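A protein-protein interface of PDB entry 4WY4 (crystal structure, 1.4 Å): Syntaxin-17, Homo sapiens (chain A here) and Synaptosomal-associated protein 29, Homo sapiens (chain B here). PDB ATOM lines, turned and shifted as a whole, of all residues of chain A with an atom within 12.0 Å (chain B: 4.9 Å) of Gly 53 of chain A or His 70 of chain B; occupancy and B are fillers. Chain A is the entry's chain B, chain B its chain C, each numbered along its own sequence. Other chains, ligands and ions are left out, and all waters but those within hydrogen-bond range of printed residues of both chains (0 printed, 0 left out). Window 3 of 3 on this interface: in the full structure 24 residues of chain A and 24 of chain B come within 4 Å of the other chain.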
ATOM      1  N   ASN A  44      -4.141   8.840  23.472  1.00  0.00           N
ATOM      2  CA  ASN A  44      -3.237   8.279  22.485  1.00  0.00           C
ATOM      3  C   ASN A  44      -2.012   9.133  22.277  1.00  0.00           C
ATOM      4  O   ASN A  44      -0.872   8.615  22.129  1.00  0.00           O
ATOM      5  CB  ASN A  44      -3.965   8.115  21.144  1.00  0.00           C
ATOM      6  CG  ASN A  44      -4.985   7.012  21.183  1.00  0.00           C
ATOM      7  OD1 ASN A  44      -4.955   6.128  22.041  1.00  0.00           O
ATOM      8  ND2 ASN A  44      -5.891   7.045  20.228  1.00  0.00           N
ATOM      9  N   VAL A  45      -2.181  10.439  22.172  1.00  0.00           N
ATOM     10  CA  VAL A  45      -1.033  11.340  21.988  1.00  0.00           C
ATOM     11  C   VAL A  45      -0.149  11.347  23.224  1.00  0.00           C
ATOM     12  O   VAL A  45       1.085  11.316  23.087  1.00  0.00           O
ATOM     13  CB  VAL A  45      -1.505  12.808  21.610  1.00  0.00           C
ATOM     14  CG1 VAL A  45      -0.350  13.813  21.636  1.00  0.00           C
ATOM     15  CG2 VAL A  45      -2.158  12.829  20.255  1.00  0.00           C
ATOM     16  N   GLU A  46      -0.711  11.286  24.408  1.00  0.00           N
ATOM     17  CA  GLU A  46       0.092  11.211  25.646  1.00  0.00           C
ATOM     18  C   GLU A  46       0.899   9.916  25.626  1.00  0.00           C
ATOM     19  O   GLU A  46       2.098   9.923  25.960  1.00  0.00           O
ATOM     20  CB  GLU A  46      -0.806  11.296  26.876  1.00  0.00           C
ATOM     21  CG  GLU A  46      -0.020  11.211  28.192  1.00  0.00           C
ATOM     22  CD  GLU A  46      -0.965  11.303  29.332  1.00  0.00           C
ATOM     23  OE1 GLU A  46      -1.589  10.274  29.675  1.00  0.00           O
ATOM     24  OE2 GLU A  46      -1.139  12.414  29.853  1.00  0.00           O
ATOM     25  N   GLU A  47       0.284   8.794  25.284  1.00  0.00           N
ATOM     26  CA  GLU A  47       0.984   7.514  25.271  1.00  0.00           C
ATOM     27  C   GLU A  47       2.083   7.524  24.218  1.00  0.00           C
ATOM     28  O   GLU A  47       3.207   7.038  24.459  1.00  0.00           O
ATOM     29  CB  GLU A  47      -0.003   6.366  25.022  1.00  0.00           C
ATOM     30  CG  GLU A  47       0.595   4.974  25.171  1.00  0.00           C
ATOM     31  CD  GLU A  47      -0.457   3.904  25.415  1.00  0.00           C
ATOM     32  OE1 GLU A  47      -1.643   4.256  25.604  1.00  0.00           O
ATOM     33  OE2 GLU A  47      -0.095   2.706  25.426  1.00  0.00           O
ATOM     34  N   GLY A  48       1.806   8.088  23.047  1.00  0.00           N
ATOM     35  CA  GLY A  48       2.842   8.158  22.029  1.00  0.00           C
ATOM     36  C   GLY A  48       4.005   9.010  22.506  1.00  0.00           C
ATOM     37  O   GLY A  48       5.184   8.666  22.265  1.00  0.00           O
ATOM     38  N   THR A  49       3.733  10.149  23.094  1.00  0.00           N
ATOM     39  CA  THR A  49       4.767  11.028  23.628  1.00  0.00           C
ATOM     40  C   THR A  49       5.611  10.298  24.652  1.00  0.00           C
ATOM     41  O   THR A  49       6.858  10.383  24.612  1.00  0.00           O
ATOM     42  CB  THR A  49       4.112  12.303  24.249  1.00  0.00           C
ATOM     43  OG1 THR A  49       3.371  12.974  23.223  1.00  0.00           O
ATOM     44  CG2 THR A  49       5.181  13.234  24.774  1.00  0.00           C
ATOM     45  N   LYS A  50       4.992   9.511  25.522  1.00  0.00           N
ATOM     46  CA  LYS A  50       5.726   8.783  26.555  1.00  0.00           C
ATOM     47  C   LYS A  50       6.619   7.722  25.920  1.00  0.00           C
ATOM     48  O   LYS A  50       7.748   7.491  26.383  1.00  0.00           O
ATOM     49  CB  LYS A  50       4.761   8.128  27.538  1.00  0.00           C
ATOM     50  CG  LYS A  50       4.189   9.105  28.529  1.00  0.00           C
ATOM     51  CD  LYS A  50       3.286   8.376  29.491  1.00  0.00           C
ATOM     52  CE  LYS A  50       2.267   9.305  30.074  1.00  0.00           C
ATOM     53  NZ  LYS A  50       1.147   8.541  30.684  1.00  0.00           N
ATOM     54  N   ASN A  51       6.152   7.067  24.862  1.00  0.00           N
ATOM     55  CA  ASN A  51       6.966   6.077  24.165  1.00  0.00           C
ATOM     56  C   ASN A  51       8.167   6.768  23.540  1.00  0.00           C
ATOM     57  O   ASN A  51       9.284   6.235  23.600  1.00  0.00           O
ATOM     58  CB  ASN A  51       6.163   5.353  23.070  1.00  0.00           C
ATOM     59  CG  ASN A  51       5.400   4.099  23.551  1.00  0.00           C
ATOM     60  OD1 ASN A  51       5.964   2.974  23.629  1.00  0.00           O
ATOM     61  ND2 ASN A  51       4.117   4.233  23.688  1.00  0.00           N
ATOM     62  N   LEU A  52       8.009   7.927  22.917  1.00  0.00           N
ATOM     63  CA  LEU A  52       9.150   8.643  22.339  1.00  0.00           C
ATOM     64  C   LEU A  52      10.112   9.063  23.453  1.00  0.00           C
ATOM     65  O   LEU A  52      11.340   9.023  23.244  1.00  0.00           O
ATOM     66  CB  LEU A  52       8.705   9.867  21.551  1.00  0.00           C
ATOM     67  CG  LEU A  52       7.885   9.582  20.295  1.00  0.00           C
ATOM     68  CD1 LEU A  52       7.387  10.915  19.721  1.00  0.00           C
ATOM     69  CD2 LEU A  52       8.680   8.758  19.277  1.00  0.00           C
ATOM     70  N   GLY A  53       9.618   9.461  24.615  1.00  0.00           N
ATOM     71  CA  GLY A  53      10.495   9.854  25.714  1.00  0.00           C
ATOM     72  C   GLY A  53      11.327   8.679  26.193  1.00  0.00           C
ATOM     73  O   GLY A  53      12.510   8.840  26.515  1.00  0.00           O
ATOM     74  N   LYS A  54      10.742   7.488  26.228  1.00  0.00           N
ATOM     75  CA  LYS A  54      11.493   6.299  26.610  1.00  0.00           C
ATOM     76  C   LYS A  54      12.566   6.005  25.593  1.00  0.00           C
ATOM     77  O   LYS A  54      13.717   5.699  25.967  1.00  0.00           O
ATOM     78  CB  LYS A  54      10.554   5.103  26.790  1.00  0.00           C
ATOM     79  CG  LYS A  54       9.652   5.274  28.006  1.00  0.00           C
ATOM     80  CD  LYS A  54       8.694   4.110  28.238  1.00  0.00           C
ATOM     81  CE  LYS A  54       8.138   4.171  29.656  1.00  0.00           C
ATOM     82  NZ  LYS A  54       7.152   3.084  29.937  1.00  0.00           N
ATOM     83  N   ALA A  55      12.235   6.097  24.316  1.00  0.00           N
ATOM     84  CA  ALA A  55      13.224   5.820  23.283  1.00  0.00           C
ATOM     85  C   ALA A  55      14.377   6.804  23.371  1.00  0.00           C
ATOM     86  O   ALA A  55      15.537   6.431  23.103  1.00  0.00           O
ATOM     87  CB  ALA A  55      12.569   5.871  21.891  1.00  0.00           C
ATOM     88  N   ALA A  56      14.086   8.056  23.716  1.00  0.00           N
ATOM     89  CA  ALA A  56      15.108   9.091  23.875  1.00  0.00           C
ATOM     90  C   ALA A  56      16.079   8.807  25.028  1.00  0.00           C
ATOM     91  O   ALA A  56      17.149   9.398  25.042  1.00  0.00           O
ATOM     92  CB  ALA A  56      14.444  10.473  24.075  1.00  0.00           C
ATOM     93  N   LYS A  57      15.716   7.926  25.964  1.00  0.00           N
ATOM     94  CA  LYS A  57      16.563   7.596  27.120  1.00  0.00           C
ATOM     95  C   LYS A  57      17.381   6.325  26.922  1.00  0.00           C
ATOM     96  O   LYS A  57      18.350   6.142  27.658  1.00  0.00           O
ATOM     97  CB  LYS A  57      15.760   7.370  28.387  1.00  0.00           C
ATOM     98  CG  LYS A  57      14.762   8.374  28.732  1.00  0.00           C
ATOM     99  CD  LYS A  57      15.297   9.664  29.234  1.00  0.00           C
ATOM    100  CE  LYS A  57      14.123  10.652  29.572  1.00  0.00           C
ATOM    101  NZ  LYS A  57      13.245  10.989  28.385  1.00  0.00           N
ATOM    102  N   TYR A  58      16.942   5.414  26.049  1.00  0.00           N
ATOM    103  CA  TYR A  58      17.551   4.093  25.878  1.00  0.00           C
ATOM    104  C   TYR A  58      18.983   4.331  25.427  1.00  0.00           C
ATOM    105  O   TYR A  58      19.256   5.359  24.792  1.00  0.00           O
ATOM    106  CB  TYR A  58      16.794   3.211  24.852  1.00  0.00           C
ATOM    107  CG  TYR A  58      15.395   2.733  25.246  1.00  0.00           C
ATOM    108  CD1 TYR A  58      15.043   2.513  26.573  1.00  0.00           C
ATOM    109  CD2 TYR A  58      14.416   2.510  24.272  1.00  0.00           C
ATOM    110  CE1 TYR A  58      13.754   2.085  26.922  1.00  0.00           C
ATOM    111  CE2 TYR A  58      13.129   2.086  24.611  1.00  0.00           C
ATOM    112  CZ  TYR A  58      12.807   1.874  25.940  1.00  0.00           C
ATOM    113  OH  TYR A  58      11.535   1.454  26.271  1.00  0.00           O
ATOM    114  OXT TYR A  58      19.878   3.523  25.691  1.00  0.00           O
ATOM    115  N   ILE B  66       6.509  18.404  23.208  1.00  0.00           N
ATOM    116  CA  ILE B  66       7.397  17.534  23.989  1.00  0.00           C
ATOM    117  C   ILE B  66       7.890  16.425  23.069  1.00  0.00           C
ATOM    118  O   ILE B  66       9.092  16.108  23.051  1.00  0.00           O
ATOM    119  CB  ILE B  66       6.660  16.978  25.198  1.00  0.00           C
ATOM    120  CG1 ILE B  66       6.342  18.125  26.169  1.00  0.00           C
ATOM    121  CG2 ILE B  66       7.460  15.854  25.858  1.00  0.00           C
ATOM    122  CD1 ILE B  66       5.354  17.766  27.206  1.00  0.00           C
ATOM    123  N   SER B  67       6.999  15.878  22.230  1.00  0.00           N
ATOM    124  CA  SER B  67       7.417  14.839  21.298  1.00  0.00           C
ATOM    125  C   SER B  67       8.474  15.300  20.326  1.00  0.00           C
ATOM    126  O   SER B  67       9.405  14.542  20.003  1.00  0.00           O
ATOM    127  CB  SER B  67       6.219  14.326  20.493  1.00  0.00           C
ATOM    128  OG  SER B  67       5.388  13.489  21.277  1.00  0.00           O
ATOM    129  N   GLN B  68       8.372  16.528  19.836  1.00  0.00           N
ATOM    130  CA  GLN B  68       9.386  17.049  18.929  1.00  0.00           C
ATOM    131  C   GLN B  68      10.745  17.151  19.631  1.00  0.00           C
ATOM    132  O   GLN B  68      11.779  16.859  19.009  1.00  0.00           O
ATOM    133  CB  GLN B  68       8.977  18.417  18.358  1.00  0.00           C
ATOM    134  CG  GLN B  68      10.008  18.994  17.360  1.00  0.00           C
ATOM    135  CD  GLN B  68      10.113  18.170  16.082  1.00  0.00           C
ATOM    136  OE1 GLN B  68       9.184  18.155  15.298  1.00  0.00           O
ATOM    137  NE2 GLN B  68      11.234  17.486  15.868  1.00  0.00           N
ATOM    138  N   LYS B  69      10.753  17.528  20.907  1.00  0.00           N
ATOM    139  CA  LYS B  69      12.009  17.544  21.671  1.00  0.00           C
ATOM    140  C   LYS B  69      12.561  16.124  21.767  1.00  0.00           C
ATOM    141  O   LYS B  69      13.784  15.924  21.612  1.00  0.00           O
ATOM    142  CB  LYS B  69      11.786  18.130  23.049  1.00  0.00           C
ATOM    143  CG  LYS B  69      11.597  19.640  23.060  1.00  0.00           C
ATOM    144  CD  LYS B  69      11.358  20.174  24.477  1.00  0.00           C
ATOM    145  CE  LYS B  69      11.272  21.698  24.507  1.00  0.00           C
ATOM    146  NZ  LYS B  69      10.186  22.230  23.652  1.00  0.00           N
ATOM    147  N   HIS B  70      11.711  15.120  21.967  1.00  0.00           N
ATOM    148  CA  HIS B  70      12.211  13.738  21.992  1.00  0.00           C
ATOM    149  C   HIS B  70      12.750  13.298  20.648  1.00  0.00           C
ATOM    150  O   HIS B  70      13.774  12.635  20.585  1.00  0.00           O
ATOM    151  CB  HIS B  70      11.124  12.754  22.409  1.00  0.00           C
ATOM    152  CG  HIS B  70      10.630  12.945  23.800  1.00  0.00           C
ATOM    153  ND1 HIS B  70      11.426  13.400  24.832  1.00  0.00           N
ATOM    154  CD2 HIS B  70       9.396  12.746  24.342  1.00  0.00           C
ATOM    155  CE1 HIS B  70      10.718  13.443  25.943  1.00  0.00           C
ATOM    156  NE2 HIS B  70       9.483  13.062  25.675  1.00  0.00           N
ATOM    157  N   ILE B  71      12.085  13.626  19.550  1.00  0.00           N
ATOM    158  CA  ILE B  71      12.580  13.307  18.220  1.00  0.00           C
ATOM    159  C   ILE B  71      13.971  13.935  18.036  1.00  0.00           C
ATOM    160  O   ILE B  71      14.920  13.261  17.585  1.00  0.00           O
ATOM    161  CB  ILE B  71      11.601  13.808  17.122  1.00  0.00           C
ATOM    162  CG1 ILE B  71      10.302  12.981  17.165  1.00  0.00           C
ATOM    163  CG2 ILE B  71      12.295  13.810  15.744  1.00  0.00           C
ATOM    164  CD1 ILE B  71       9.136  13.632  16.388  1.00  0.00           C
ATOM    165  N   ASN B  72      14.130  15.193  18.429  1.00  0.00           N
ATOM    166  CA  ASN B  72      15.442  15.856  18.313  1.00  0.00           C
ATOM    167  C   ASN B  72      16.504  15.122  19.138  1.00  0.00           C
ATOM    168  O   ASN B  72      17.645  14.960  18.699  1.00  0.00           O
ATOM    169  CB  ASN B  72      15.368  17.308  18.772  1.00  0.00           C
ATOM    170  CG  ASN B  72      14.480  18.183  17.887  1.00  0.00           C
ATOM    171  OD1 ASN B  72      14.121  17.809  16.762  1.00  0.00           O
ATOM    172  ND2 ASN B  72      14.134  19.371  18.395  1.00  0.00           N
ATOM    173  N   SER B  73      16.142  14.672  20.329  1.00  0.00           N
ATOM    174  CA  SER B  73      17.092  13.919  21.180  1.00  0.00           C
ATOM    175  C   SER B  73      17.490  12.605  20.547  1.00  0.00           C
ATOM    176  O   SER B  73      18.679  12.210  20.571  1.00  0.00           O
ATOM    177  CB  SER B  73      16.430  13.655  22.529  1.00  0.00           C
ATOM    178  OG  SER B  73      16.206  14.864  23.216  1.00  0.00           O
ATOM    179  N   ILE B  74      16.525  11.899  19.977  1.00  0.00           N
ATOM    180  CA  ILE B  74      16.796  10.600  19.388  1.00  0.00           C
ATOM    181  C   ILE B  74      17.720  10.742  18.179  1.00  0.00           C
ATOM    182  O   ILE B  74      18.640   9.918  17.977  1.00  0.00           O
ATOM    183  CB  ILE B  74      15.471   9.894  18.979  1.00  0.00           C
ATOM    184  CG1 ILE B  74      14.663   9.533  20.230  1.00  0.00           C
ATOM    185  CG2 ILE B  74      15.793   8.647  18.167  1.00  0.00           C
ATOM    186  CD1 ILE B  74      13.192   9.201  19.951  1.00  0.00           C
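The side-chain hydroxyl of Ser 67 of chain B is in hydrogen-bond range of the side-chain hydroxyl of Thr 49 of chain A (2.8 Å).
OG1 of Thr 49 of chain A is in hydrogen-bond range of O of Val 45 of chain A (2.8 Å). NZ of Lys 57 of chain A sits at hydrogen-bond distance from O of Gly 53 of chain A.
Thr 49 of chain A touches Ile 66 of chain B. Thr 49 of chain A touches His 70 of chain B (O to CD2, 3.5 Å). Leu 52 of chain A touches Ser 67 of chain B (CD1 to OG, 3.6 Å). O of Leu 52 of chain A touches CB of His 70 of chain B, 3.8 Å away. O of Leu 52 of chain A touches CD1 of Ile 74 of chain B, at 3.8 Å. Gly 53 of chain A touches His 70 of chain B (N to CD2, 3.3 Å). CB of Ala 55 of chain A touches CD1 of Ile 74 of chain B, at 3.9 Å. Ile 74 of chain B touches Ala 56 of chain A.
Of chain B, only His 70 comes within 4 Å of Gly 53 of chain A. His 70 of chain B touches just these residues of chain A: Thr 49 (3.5 Å), Leu 52 (3.8 Å) and Gly 53 (3.3 Å). Of chain A, only Thr 49 (3.6 Å) comes within 4 Å of Ile 66 of chain B. Ser 67 of chain B touches just these residues of chain A: Thr 49 and Leu 52. Lys 69 of chain B touches none of the printed residues of chain A. No residue of chain A comes within 4 Å of Ile 71 of chain B. No residue of chain A comes within 4 Å of Asn 72 of chain B. Of chain A, only Leu 52 (3.8 Å), Ala 55 (3.9 Å) and Ala 56 (3.7 Å) come within 4 Å of Ile 74 of chain B. Of the printed residues of chain B, Ala 55 of chain A touches Ile 74. Printed residues of chain B within 4 Å of Thr 49 of chain A: Ile 66, Ser 67 and His 70. Of the printed residues of chain B, Ala 56 of chain A touches Ile 74 (3.7 Å). Printed residues of chain B within 4 Å of Leu 52 of chain A: Ser 67, His 70 and Ile 74. Val 45 of chain A touches none of the printed residues of chain B. Glu 46 of chain A touches none of the printed residues of chain B. The nearest printed residue of chain B that does not touch Gly 53 of chain A is Ile 74 of chain B (5.9 Å). The nearest residue of chain A that does not touch His 70 of chain B is Ala 56 of chain A (4.2 Å). The nearest printed residue of chain B that does not touch Ala 56 of chain A is Ser 73 of chain B (4.1 Å).
Hydrophobic or aromatic side chains of chain A within 4 Å of the printed part of chain B: Leu 52, Ala 55 and Ala 56. Along chain A the printed residues that touch a printed residue of chain B span positions 49 to 56. Hydrophobic or aromatic side chains of chain B within 4 Å of the printed part of chain A: Ile 66, His 70 and Ile 74. Among the printed residues, no Asp or Glu carboxylate lies within 4 Å of a Lys or Arg side-chain nitrogen of the other chain.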
